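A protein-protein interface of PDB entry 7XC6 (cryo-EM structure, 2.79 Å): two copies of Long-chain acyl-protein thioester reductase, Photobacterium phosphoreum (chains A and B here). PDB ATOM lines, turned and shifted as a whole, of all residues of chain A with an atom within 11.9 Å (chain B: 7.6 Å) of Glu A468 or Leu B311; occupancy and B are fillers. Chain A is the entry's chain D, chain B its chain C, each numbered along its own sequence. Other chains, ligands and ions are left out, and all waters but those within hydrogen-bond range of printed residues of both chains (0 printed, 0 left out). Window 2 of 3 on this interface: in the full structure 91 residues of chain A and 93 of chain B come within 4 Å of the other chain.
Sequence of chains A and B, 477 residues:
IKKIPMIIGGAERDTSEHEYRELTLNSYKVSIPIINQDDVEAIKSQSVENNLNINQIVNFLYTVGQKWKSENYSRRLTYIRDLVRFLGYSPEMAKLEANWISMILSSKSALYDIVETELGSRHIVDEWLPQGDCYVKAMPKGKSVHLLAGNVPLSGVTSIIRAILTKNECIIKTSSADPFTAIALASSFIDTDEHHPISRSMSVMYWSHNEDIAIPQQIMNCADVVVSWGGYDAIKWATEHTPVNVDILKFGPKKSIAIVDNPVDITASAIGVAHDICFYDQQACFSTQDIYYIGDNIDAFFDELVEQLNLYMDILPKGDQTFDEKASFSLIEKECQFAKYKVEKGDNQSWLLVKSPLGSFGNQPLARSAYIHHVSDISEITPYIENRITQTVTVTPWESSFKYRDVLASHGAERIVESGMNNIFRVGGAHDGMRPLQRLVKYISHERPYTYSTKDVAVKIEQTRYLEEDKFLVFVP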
ATOM      1  N   LYS A 460       2.362  19.572 -24.621  1.00  0.00           N
ATOM      2  CA  LYS A 460       2.619  18.608 -23.561  1.00  0.00           C
ATOM      3  C   LYS A 460       3.931  17.884 -23.826  1.00  0.00           C
ATOM      4  O   LYS A 460       4.239  17.518 -24.961  1.00  0.00           O
ATOM      5  CB  LYS A 460       1.466  17.616 -23.461  1.00  0.00           C
ATOM      6  CG  LYS A 460       0.178  18.252 -22.992  1.00  0.00           C
ATOM      7  CD  LYS A 460      -0.924  17.234 -22.825  1.00  0.00           C
ATOM      8  CE  LYS A 460      -2.266  17.922 -22.670  1.00  0.00           C
ATOM      9  NZ  LYS A 460      -3.333  16.971 -22.263  1.00  0.00           N
ATOM     10  N   ILE A 461       4.705  17.679 -22.766  1.00  0.00           N
ATOM     11  CA  ILE A 461       6.102  17.242 -22.909  1.00  0.00           C
ATOM     12  C   ILE A 461       6.078  15.723 -22.979  1.00  0.00           C
ATOM     13  O   ILE A 461       6.255  15.008 -21.991  1.00  0.00           O
ATOM     14  CB  ILE A 461       6.984  17.771 -21.778  1.00  0.00           C
ATOM     15  CG1 ILE A 461       6.728  19.263 -21.571  1.00  0.00           C
ATOM     16  CG2 ILE A 461       8.438  17.522 -22.092  1.00  0.00           C
ATOM     17  CD1 ILE A 461       7.215  19.789 -20.255  1.00  0.00           C
ATOM     18  N   GLU A 462       5.872  15.213 -24.186  1.00  0.00           N
ATOM     19  CA  GLU A 462       5.892  13.782 -24.462  1.00  0.00           C
ATOM     20  C   GLU A 462       7.148  13.505 -25.280  1.00  0.00           C
ATOM     21  O   GLU A 462       7.116  13.504 -26.509  1.00  0.00           O
ATOM     22  CB  GLU A 462       4.639  13.349 -25.199  1.00  0.00           C
ATOM     23  CG  GLU A 462       3.376  14.004 -24.695  1.00  0.00           C
ATOM     24  CD  GLU A 462       2.131  13.384 -25.283  1.00  0.00           C
ATOM     25  OE1 GLU A 462       2.202  12.225 -25.736  1.00  0.00           O
ATOM     26  OE2 GLU A 462       1.080  14.055 -25.296  1.00  0.00           O
ATOM     27  N   GLN A 463       8.258  13.265 -24.587  1.00  0.00           N
ATOM     28  CA  GLN A 463       9.533  13.138 -25.281  1.00  0.00           C
ATOM     29  C   GLN A 463       9.618  11.849 -26.086  1.00  0.00           C
ATOM     30  O   GLN A 463      10.240  11.831 -27.153  1.00  0.00           O
ATOM     31  CB  GLN A 463      10.679  13.224 -24.279  1.00  0.00           C
ATOM     32  CG  GLN A 463      10.487  14.305 -23.238  1.00  0.00           C
ATOM     33  CD  GLN A 463      11.740  14.565 -22.442  1.00  0.00           C
ATOM     34  OE1 GLN A 463      12.823  14.712 -23.001  1.00  0.00           O
ATOM     35  NE2 GLN A 463      11.602  14.620 -21.126  1.00  0.00           N
ATOM     36  N   THR A 464       8.991  10.774 -25.611  1.00  0.00           N
ATOM     37  CA  THR A 464       9.010   9.523 -26.361  1.00  0.00           C
ATOM     38  C   THR A 464       8.187   9.641 -27.635  1.00  0.00           C
ATOM     39  O   THR A 464       8.623   9.214 -28.712  1.00  0.00           O
ATOM     40  CB  THR A 464       8.486   8.382 -25.494  1.00  0.00           C
ATOM     41  OG1 THR A 464       9.226   8.334 -24.271  1.00  0.00           O
ATOM     42  CG2 THR A 464       8.630   7.059 -26.216  1.00  0.00           C
ATOM     43  N   ARG A 465       6.987  10.214 -27.527  1.00  0.00           N
ATOM     44  CA  ARG A 465       6.120  10.359 -28.689  1.00  0.00           C
ATOM     45  C   ARG A 465       6.798  11.159 -29.790  1.00  0.00           C
ATOM     46  O   ARG A 465       6.662  10.836 -30.975  1.00  0.00           O
ATOM     47  CB  ARG A 465       4.808  11.022 -28.281  1.00  0.00           C
ATOM     48  CG  ARG A 465       3.833  11.198 -29.421  1.00  0.00           C
ATOM     49  CD  ARG A 465       2.678  12.087 -29.021  1.00  0.00           C
ATOM     50  NE  ARG A 465       2.254  12.951 -30.114  1.00  0.00           N
ATOM     51  CZ  ARG A 465       1.300  13.867 -30.009  1.00  0.00           C
ATOM     52  NH1 ARG A 465       0.975  14.613 -31.054  1.00  0.00           N
ATOM     53  NH2 ARG A 465       0.668  14.035 -28.858  1.00  0.00           N
ATOM     54  N   TYR A 466       7.540  12.195 -29.422  1.00  0.00           N
ATOM     55  CA  TYR A 466       8.202  13.039 -30.403  1.00  0.00           C
ATOM     56  C   TYR A 466       9.567  12.512 -30.815  1.00  0.00           C
ATOM     57  O   TYR A 466      10.087  12.935 -31.850  1.00  0.00           O
ATOM     58  CB  TYR A 466       8.327  14.461 -29.856  1.00  0.00           C
ATOM     59  CG  TYR A 466       6.985  15.111 -29.648  1.00  0.00           C
ATOM     60  CD1 TYR A 466       5.989  14.998 -30.602  1.00  0.00           C
ATOM     61  CD2 TYR A 466       6.701  15.812 -28.489  1.00  0.00           C
ATOM     62  CE1 TYR A 466       4.760  15.577 -30.418  1.00  0.00           C
ATOM     63  CE2 TYR A 466       5.471  16.394 -28.295  1.00  0.00           C
ATOM     64  CZ  TYR A 466       4.504  16.273 -29.264  1.00  0.00           C
ATOM     65  OH  TYR A 466       3.272  16.851 -29.082  1.00  0.00           O
ATOM     66  N   LEU A 467      10.155  11.598 -30.043  1.00  0.00           N
ATOM     67  CA  LEU A 467      11.328  10.887 -30.530  1.00  0.00           C
ATOM     68  C   LEU A 467      10.938   9.854 -31.575  1.00  0.00           C
ATOM     69  O   LEU A 467      11.701   9.590 -32.509  1.00  0.00           O
ATOM     70  CB  LEU A 467      12.069  10.222 -29.375  1.00  0.00           C
ATOM     71  CG  LEU A 467      13.260  10.984 -28.800  1.00  0.00           C
ATOM     72  CD1 LEU A 467      13.817  10.245 -27.605  1.00  0.00           C
ATOM     73  CD2 LEU A 467      14.329  11.172 -29.855  1.00  0.00           C
ATOM     74  N   GLU A 468       9.757   9.254 -31.426  1.00  0.00           N
ATOM     75  CA  GLU A 468       9.238   8.374 -32.466  1.00  0.00           C
ATOM     76  C   GLU A 468       8.972   9.148 -33.751  1.00  0.00           C
ATOM     77  O   GLU A 468       9.485   8.801 -34.820  1.00  0.00           O
ATOM     78  CB  GLU A 468       7.964   7.686 -31.981  1.00  0.00           C
ATOM     79  CG  GLU A 468       8.192   6.647 -30.913  1.00  0.00           C
ATOM     80  CD  GLU A 468       6.916   5.941 -30.519  1.00  0.00           C
ATOM     81  OE1 GLU A 468       6.202   6.454 -29.634  1.00  0.00           O
ATOM     82  OE2 GLU A 468       6.622   4.876 -31.100  1.00  0.00           O
ATOM     83  N   GLU A 469       8.164  10.204 -33.661  1.00  0.00           N
ATOM     84  CA  GLU A 469       7.783  10.974 -34.837  1.00  0.00           C
ATOM     85  C   GLU A 469       8.909  11.841 -35.378  1.00  0.00           C
ATOM     86  O   GLU A 469       8.760  12.393 -36.472  1.00  0.00           O
ATOM     87  CB  GLU A 469       6.581  11.857 -34.517  1.00  0.00           C
ATOM     88  CG  GLU A 469       5.400  11.109 -33.948  1.00  0.00           C
ATOM     89  CD  GLU A 469       4.313  12.035 -33.460  1.00  0.00           C
ATOM     90  OE1 GLU A 469       4.617  13.215 -33.193  1.00  0.00           O
ATOM     91  OE2 GLU A 469       3.157  11.585 -33.332  1.00  0.00           O
ATOM     92  N   ASP A 470      10.013  11.984 -34.645  1.00  0.00           N
ATOM     93  CA  ASP A 470      11.136  12.829 -35.048  1.00  0.00           C
ATOM     94  C   ASP A 470      10.700  14.291 -35.177  1.00  0.00           C
ATOM     95  O   ASP A 470      10.828  14.919 -36.229  1.00  0.00           O
ATOM     96  CB  ASP A 470      11.767  12.321 -36.350  1.00  0.00           C
ATOM     97  CG  ASP A 470      13.187  12.805 -36.540  1.00  0.00           C
ATOM     98  OD1 ASP A 470      13.521  13.893 -36.031  1.00  0.00           O
ATOM     99  OD2 ASP A 470      13.968  12.104 -37.212  1.00  0.00           O
ATOM    100  N   LYS A 471      10.174  14.823 -34.077  1.00  0.00           N
ATOM    101  CA  LYS A 471       9.680  16.199 -34.016  1.00  0.00           C
ATOM    102  C   LYS A 471      10.309  16.891 -32.812  1.00  0.00           C
ATOM    103  O   LYS A 471       9.856  16.701 -31.681  1.00  0.00           O
ATOM    104  CB  LYS A 471       8.159  16.237 -33.918  1.00  0.00           C
ATOM    105  CG  LYS A 471       7.436  15.974 -35.213  1.00  0.00           C
ATOM    106  CD  LYS A 471       6.004  16.459 -35.144  1.00  0.00           C
ATOM    107  CE  LYS A 471       5.050  15.380 -35.612  1.00  0.00           C
ATOM    108  NZ  LYS A 471       5.524  14.739 -36.868  1.00  0.00           N
ATOM    109  N   PHE A 472      11.349  17.672 -33.038  1.00  0.00           N
ATOM    110  CA  PHE A 472      11.820  18.506 -31.938  1.00  0.00           C
ATOM    111  C   PHE A 472      11.883  19.983 -32.287  1.00  0.00           C
ATOM    112  O   PHE A 472      11.437  20.810 -31.490  1.00  0.00           O
ATOM    113  CB  PHE A 472      13.200  18.039 -31.464  1.00  0.00           C
ATOM    114  CG  PHE A 472      13.565  18.528 -30.093  1.00  0.00           C
ATOM    115  CD1 PHE A 472      13.924  19.847 -29.882  1.00  0.00           C
ATOM    116  CD2 PHE A 472      13.543  17.671 -29.014  1.00  0.00           C
ATOM    117  CE1 PHE A 472      14.256  20.294 -28.630  1.00  0.00           C
ATOM    118  CE2 PHE A 472      13.875  18.117 -27.758  1.00  0.00           C
ATOM    119  CZ  PHE A 472      14.232  19.430 -27.567  1.00  0.00           C
ATOM    120  N   LEU A 473      12.398  20.336 -33.462  1.00  0.00           N
ATOM    121  CA  LEU A 473      12.683  21.733 -33.758  1.00  0.00           C
ATOM    122  C   LEU A 473      11.451  22.522 -34.167  1.00  0.00           C
ATOM    123  O   LEU A 473      11.521  23.752 -34.236  1.00  0.00           O
ATOM    124  CB  LEU A 473      13.743  21.833 -34.851  1.00  0.00           C
ATOM    125  CG  LEU A 473      15.123  21.339 -34.432  1.00  0.00           C
ATOM    126  CD1 LEU A 473      16.064  21.339 -35.613  1.00  0.00           C
ATOM    127  CD2 LEU A 473      15.671  22.194 -33.307  1.00  0.00           C
ATOM    128  N   VAL A 474      10.330  21.856 -34.436  1.00  0.00           N
ATOM    129  CA  VAL A 474       9.104  22.583 -34.724  1.00  0.00           C
ATOM    130  C   VAL A 474       8.520  23.194 -33.457  1.00  0.00           C
ATOM    131  O   VAL A 474       7.748  24.157 -33.536  1.00  0.00           O
ATOM    132  CB  VAL A 474       8.096  21.650 -35.416  1.00  0.00           C
ATOM    133  CG1 VAL A 474       7.677  20.534 -34.482  1.00  0.00           C
ATOM    134  CG2 VAL A 474       6.893  22.421 -35.926  1.00  0.00           C
ATOM    135  N   PHE A 475       8.891  22.679 -32.288  1.00  0.00           N
ATOM    136  CA  PHE A 475       8.408  23.208 -31.023  1.00  0.00           C
ATOM    137  C   PHE A 475       9.339  24.243 -30.412  1.00  0.00           C
ATOM    138  O   PHE A 475       8.916  24.979 -29.515  1.00  0.00           O
ATOM    139  CB  PHE A 475       8.204  22.072 -30.019  1.00  0.00           C
ATOM    140  CG  PHE A 475       7.305  20.983 -30.513  1.00  0.00           C
ATOM    141  CD1 PHE A 475       6.037  21.272 -30.975  1.00  0.00           C
ATOM    142  CD2 PHE A 475       7.727  19.668 -30.511  1.00  0.00           C
ATOM    143  CE1 PHE A 475       5.209  20.271 -31.429  1.00  0.00           C
ATOM    144  CE2 PHE A 475       6.904  18.665 -30.964  1.00  0.00           C
ATOM    145  CZ  PHE A 475       5.644  18.967 -31.422  1.00  0.00           C
ATOM    146  N   ILE B 271       6.680   3.698 -20.447  1.00  0.00           N
ATOM    147  CA  ILE B 271       7.282   4.669 -21.358  1.00  0.00           C
ATOM    148  C   ILE B 271       8.194   5.615 -20.592  1.00  0.00           C
ATOM    149  O   ILE B 271       9.343   5.857 -20.980  1.00  0.00           O
ATOM    150  CB  ILE B 271       6.191   5.443 -22.117  1.00  0.00           C
ATOM    151  CG1 ILE B 271       5.609   4.591 -23.240  1.00  0.00           C
ATOM    152  CG2 ILE B 271       6.754   6.726 -22.687  1.00  0.00           C
ATOM    153  CD1 ILE B 271       4.317   5.129 -23.791  1.00  0.00           C
ATOM    154  N   ALA B 274      11.318   3.854 -19.085  1.00  0.00           N
ATOM    155  CA  ALA B 274      12.266   3.564 -20.155  1.00  0.00           C
ATOM    156  C   ALA B 274      12.981   4.824 -20.614  1.00  0.00           C
ATOM    157  O   ALA B 274      14.186   4.794 -20.883  1.00  0.00           O
ATOM    158  CB  ALA B 274      11.546   2.903 -21.326  1.00  0.00           C
ATOM    159  N   CYS B 278      17.014   5.255 -20.462  1.00  0.00           N
ATOM    160  CA  CYS B 278      17.735   5.282 -21.724  1.00  0.00           C
ATOM    161  C   CYS B 278      18.322   6.639 -22.081  1.00  0.00           C
ATOM    162  O   CYS B 278      19.266   6.689 -22.874  1.00  0.00           O
ATOM    163  CB  CYS B 278      16.812   4.825 -22.855  1.00  0.00           C
ATOM    164  SG  CYS B 278      16.461   3.057 -22.840  1.00  0.00           S
ATOM    165  N   LEU B 305       7.626  -2.594 -19.706  1.00  0.00           N
ATOM    166  CA  LEU B 305       8.907  -1.903 -19.696  1.00  0.00           C
ATOM    167  C   LEU B 305       9.870  -2.528 -20.689  1.00  0.00           C
ATOM    168  O   LEU B 305      10.673  -1.824 -21.304  1.00  0.00           O
ATOM    169  CB  LEU B 305       9.499  -1.921 -18.289  1.00  0.00           C
ATOM    170  CG  LEU B 305      10.710  -1.021 -18.047  1.00  0.00           C
ATOM    171  CD1 LEU B 305      10.383   0.411 -18.395  1.00  0.00           C
ATOM    172  CD2 LEU B 305      11.172  -1.127 -16.609  1.00  0.00           C
ATOM    173  N   VAL B 306       9.813  -3.848 -20.854  1.00  0.00           N
ATOM    174  CA  VAL B 306      10.631  -4.500 -21.871  1.00  0.00           C
ATOM    175  C   VAL B 306      10.247  -3.993 -23.255  1.00  0.00           C
ATOM    176  O   VAL B 306      11.110  -3.701 -24.092  1.00  0.00           O
ATOM    177  CB  VAL B 306      10.498  -6.029 -21.767  1.00  0.00           C
ATOM    178  CG1 VAL B 306      10.908  -6.691 -23.064  1.00  0.00           C
ATOM    179  CG2 VAL B 306      11.342  -6.549 -20.620  1.00  0.00           C
ATOM    180  N   GLU B 307       8.945  -3.864 -23.509  1.00  0.00           N
ATOM    181  CA  GLU B 307       8.497  -3.339 -24.798  1.00  0.00           C
ATOM    182  C   GLU B 307       8.985  -1.910 -25.018  1.00  0.00           C
ATOM    183  O   GLU B 307       9.459  -1.562 -26.107  1.00  0.00           O
ATOM    184  CB  GLU B 307       6.975  -3.404 -24.903  1.00  0.00           C
ATOM    185  CG  GLU B 307       6.404  -4.804 -24.947  1.00  0.00           C
ATOM    186  CD  GLU B 307       5.010  -4.830 -25.540  1.00  0.00           C
ATOM    187  OE1 GLU B 307       4.539  -5.920 -25.921  1.00  0.00           O
ATOM    188  OE2 GLU B 307       4.388  -3.751 -25.639  1.00  0.00           O
ATOM    189  N   GLN B 308       8.875  -1.061 -23.995  1.00  0.00           N
ATOM    190  CA  GLN B 308       9.313   0.323 -24.160  1.00  0.00           C
ATOM    191  C   GLN B 308      10.827   0.427 -24.312  1.00  0.00           C
ATOM    192  O   GLN B 308      11.318   1.289 -25.051  1.00  0.00           O
ATOM    193  CB  GLN B 308       8.837   1.176 -22.987  1.00  0.00           C
ATOM    194  CG  GLN B 308       7.330   1.273 -22.850  1.00  0.00           C
ATOM    195  CD  GLN B 308       6.603   1.220 -24.175  1.00  0.00           C
ATOM    196  OE1 GLN B 308       5.809   0.316 -24.417  1.00  0.00           O
ATOM    197  NE2 GLN B 308       6.854   2.200 -25.033  1.00  0.00           N
ATOM    198  N   LEU B 309      11.582  -0.441 -23.638  1.00  0.00           N
ATOM    199  CA  LEU B 309      13.026  -0.460 -23.829  1.00  0.00           C
ATOM    200  C   LEU B 309      13.384  -0.932 -25.230  1.00  0.00           C
ATOM    201  O   LEU B 309      14.348  -0.446 -25.825  1.00  0.00           O
ATOM    202  CB  LEU B 309      13.685  -1.345 -22.776  1.00  0.00           C
ATOM    203  CG  LEU B 309      13.715  -0.798 -21.350  1.00  0.00           C
ATOM    204  CD1 LEU B 309      13.955  -1.917 -20.361  1.00  0.00           C
ATOM    205  CD2 LEU B 309      14.773   0.275 -21.207  1.00  0.00           C
ATOM    206  N   ASN B 310      12.612  -1.870 -25.781  1.00  0.00           N
ATOM    207  CA  ASN B 310      12.826  -2.266 -27.168  1.00  0.00           C
ATOM    208  C   ASN B 310      12.512  -1.128 -28.127  1.00  0.00           C
ATOM    209  O   ASN B 310      13.160  -0.998 -29.170  1.00  0.00           O
ATOM    210  CB  ASN B 310      11.982  -3.492 -27.504  1.00  0.00           C
ATOM    211  CG  ASN B 310      12.628  -4.782 -27.054  1.00  0.00           C
ATOM    212  OD1 ASN B 310      13.850  -4.879 -26.964  1.00  0.00           O
ATOM    213  ND2 ASN B 310      11.809  -5.785 -26.773  1.00  0.00           N
ATOM    214  N   LEU B 311      11.519  -0.303 -27.800  1.00  0.00           N
ATOM    215  CA  LEU B 311      11.242   0.878 -28.614  1.00  0.00           C
ATOM    216  C   LEU B 311      12.407   1.860 -28.574  1.00  0.00           C
ATOM    217  O   LEU B 311      12.852   2.365 -29.613  1.00  0.00           O
ATOM    218  CB  LEU B 311       9.956   1.551 -28.141  1.00  0.00           C
ATOM    219  CG  LEU B 311       9.698   2.943 -28.708  1.00  0.00           C
ATOM    220  CD1 LEU B 311       9.218   2.855 -30.140  1.00  0.00           C
ATOM    221  CD2 LEU B 311       8.688   3.676 -27.852  1.00  0.00           C
ATOM    222  N   TYR B 312      12.902   2.156 -27.373  1.00  0.00           N
ATOM    223  CA  TYR B 312      14.061   3.034 -27.238  1.00  0.00           C
ATOM    224  C   TYR B 312      15.317   2.436 -27.854  1.00  0.00           C
ATOM    225  O   TYR B 312      16.248   3.180 -28.176  1.00  0.00           O
ATOM    226  CB  TYR B 312      14.293   3.369 -25.768  1.00  0.00           C
ATOM    227  CG  TYR B 312      13.531   4.591 -25.336  1.00  0.00           C
ATOM    228  CD1 TYR B 312      14.049   5.858 -25.544  1.00  0.00           C
ATOM    229  CD2 TYR B 312      12.270   4.484 -24.778  1.00  0.00           C
ATOM    230  CE1 TYR B 312      13.355   6.978 -25.173  1.00  0.00           C
ATOM    231  CE2 TYR B 312      11.565   5.599 -24.409  1.00  0.00           C
ATOM    232  CZ  TYR B 312      12.113   6.844 -24.608  1.00  0.00           C
ATOM    233  OH  TYR B 312      11.420   7.967 -24.242  1.00  0.00           O
ATOM    234  N   MET B 313      15.371   1.116 -28.011  1.00  0.00           N
ATOM    235  CA  MET B 313      16.468   0.498 -28.745  1.00  0.00           C
ATOM    236  C   MET B 313      16.551   1.022 -30.171  1.00  0.00           C
ATOM    237  O   MET B 313      17.635   1.043 -30.763  1.00  0.00           O
ATOM    238  CB  MET B 313      16.294  -1.018 -28.752  1.00  0.00           C
ATOM    239  CG  MET B 313      17.494  -1.788 -29.243  1.00  0.00           C
ATOM    240  SD  MET B 313      17.292  -3.553 -28.983  1.00  0.00           S
ATOM    241  CE  MET B 313      15.744  -3.815 -29.835  1.00  0.00           C
ATOM    242  N   ASP B 314      15.426   1.448 -30.733  1.00  0.00           N
ATOM    243  CA  ASP B 314      15.359   1.919 -32.109  1.00  0.00           C
ATOM    244  C   ASP B 314      15.276   3.429 -32.229  1.00  0.00           C
ATOM    245  O   ASP B 314      15.953   4.009 -33.077  1.00  0.00           O
ATOM    246  CB  ASP B 314      14.153   1.297 -32.818  1.00  0.00           C
ATOM    247  CG  ASP B 314      14.082  -0.201 -32.638  1.00  0.00           C
ATOM    248  OD1 ASP B 314      15.034  -0.896 -33.048  1.00  0.00           O
ATOM    249  OD2 ASP B 314      13.074  -0.687 -32.084  1.00  0.00           O
ATOM    250  N   ILE B 315      14.466   4.089 -31.400  1.00  0.00           N
ATOM    251  CA  ILE B 315      14.306   5.532 -31.555  1.00  0.00           C
ATOM    252  C   ILE B 315      15.438   6.324 -30.911  1.00  0.00           C
ATOM    253  O   ILE B 315      15.566   7.524 -31.178  1.00  0.00           O
ATOM    254  CB  ILE B 315      12.955   6.000 -30.993  1.00  0.00           C
ATOM    255  CG1 ILE B 315      12.927   5.856 -29.474  1.00  0.00           C
ATOM    256  CG2 ILE B 315      11.823   5.231 -31.633  1.00  0.00           C
ATOM    257  CD1 ILE B 315      11.678   6.406 -28.838  1.00  0.00           C
ATOM    258  N   LEU B 316      16.262   5.698 -30.078  1.00  0.00           N
ATOM    259  CA  LEU B 316      17.389   6.378 -29.436  1.00  0.00           C
ATOM    260  C   LEU B 316      18.428   5.340 -29.052  1.00  0.00           C
ATOM    261  O   LEU B 316      18.543   4.947 -27.885  1.00  0.00           O
ATOM    262  CB  LEU B 316      16.930   7.173 -28.213  1.00  0.00           C
ATOM    263  CG  LEU B 316      17.915   8.179 -27.617  1.00  0.00           C
ATOM    264  CD1 LEU B 316      18.004   9.423 -28.477  1.00  0.00           C
ATOM    265  CD2 LEU B 316      17.505   8.540 -26.204  1.00  0.00           C
ATOM    266  N   PRO B 317      19.216   4.875 -30.013  1.00  0.00           N
ATOM    267  CA  PRO B 317      20.125   3.751 -29.746  1.00  0.00           C
ATOM    268  C   PRO B 317      21.291   4.104 -28.836  1.00  0.00           C
ATOM    269  O   PRO B 317      21.485   5.264 -28.468  1.00  0.00           O
ATOM    270  CB  PRO B 317      20.616   3.345 -31.142  1.00  0.00           C
ATOM    271  CG  PRO B 317      19.924   4.218 -32.116  1.00  0.00           C
ATOM    272  CD  PRO B 317      19.276   5.341 -31.405  1.00  0.00           C
ATOM    273  N   TRP B 351      19.943  -3.170 -23.585  1.00  0.00           N
ATOM    274  CA  TRP B 351      19.453  -2.828 -22.261  1.00  0.00           C
ATOM    275  C   TRP B 351      19.446  -4.083 -21.403  1.00  0.00           C
ATOM    276  O   TRP B 351      19.722  -5.186 -21.875  1.00  0.00           O
ATOM    277  CB  TRP B 351      18.060  -2.195 -22.325  1.00  0.00           C
ATOM    278  CG  TRP B 351      17.093  -2.960 -23.161  1.00  0.00           C
ATOM    279  CD1 TRP B 351      16.826  -2.769 -24.481  1.00  0.00           C
ATOM    280  CD2 TRP B 351      16.254  -4.038 -22.735  1.00  0.00           C
ATOM    281  NE1 TRP B 351      15.877  -3.661 -24.906  1.00  0.00           N
ATOM    282  CE2 TRP B 351      15.509  -4.451 -23.851  1.00  0.00           C
ATOM    283  CE3 TRP B 351      16.063  -4.693 -21.517  1.00  0.00           C
ATOM    284  CZ2 TRP B 351      14.591  -5.489 -23.788  1.00  0.00           C
ATOM    285  CZ3 TRP B 351      15.151  -5.721 -21.457  1.00  0.00           C
ATOM    286  CH2 TRP B 351      14.426  -6.110 -22.584  1.00  0.00           C
ATOM    287  N   ARG B 368      22.619   0.359 -19.863  1.00  0.00           N
ATOM    288  CA  ARG B 368      21.211   0.715 -19.733  1.00  0.00           C
ATOM    289  C   ARG B 368      20.537  -0.149 -18.679  1.00  0.00           C
ATOM    290  O   ARG B 368      19.323  -0.372 -18.742  1.00  0.00           O
ATOM    291  CB  ARG B 368      20.482   0.626 -21.074  1.00  0.00           C
ATOM    292  CG  ARG B 368      20.241   1.991 -21.712  1.00  0.00           C
ATOM    293  CD  ARG B 368      20.251   1.918 -23.223  1.00  0.00           C
ATOM    294  NE  ARG B 368      20.508   3.212 -23.846  1.00  0.00           N
ATOM    295  CZ  ARG B 368      19.772   3.728 -24.824  1.00  0.00           C
ATOM    296  NH1 ARG B 368      18.732   3.060 -25.297  1.00  0.00           N
ATOM    297  NH2 ARG B 368      20.078   4.910 -25.335  1.00  0.00           N
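Thr A464 touches Ile B271 (OG1 to CG2, 3.3 Å). Thr A464 touches Leu B311. Leu A467 touches Ile B315. Glu A468 touches Leu B311 (OE2 to CD1, 3.4 Å). Ile B315 touches Glu A468.
Of chain A, only Thr A464 and Glu A468 come within 4 Å of Leu B311. Of the printed residues of chain A, Ile B271 touches Thr A464. No residue of chain A comes within 4 Å of Gln B308. No residue of chain A comes within 4 Å of Asn B310. Tyr B312 touches one residue of chain A. No residue of chain A comes within 4 Å of Met B313. Ile B315 touches just these residues of chain A: Leu A467 (3.9 Å) and Glu A468 (3.96 Å). Printed residues of chain B within 4 Å of Thr A464: Ile B271, Leu B311 and Tyr B312. Of the printed residues of chain B, Leu A467 touches Ile B315 (3.9 Å). Lys A460 touches none of the printed residues of chain B. The nearest printed residue of chain B that does not touch Glu A468 is Ile B271 (6.3 Å).
The side-chain hydroxyl (OG1) of Thr A464 sits close to the side-chain hydroxyl (OH) of Tyr B312, at 2.2 Å.
No position is printed for both chains. Of the 6 pairs that touch across the chains among the printed residues, none has its exchanged pair printed and touching as well.
Printed residues of chain B that touch a printed residue of chain A: Ile B271, Leu B311, Tyr B312 and Ile B315. Hydrophobic or aromatic side chains of chain B within 4 Å of the printed part of chain A: Ile B271, Leu B311, Tyr B312 and Ile B315. Of the 16 printed residues of chain A, 3 touch a printed residue of chain B. Among the printed residues, no Asp or Glu carboxylate lies within 4 Å of a Lys or Arg side-chain nitrogen of the other chain.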
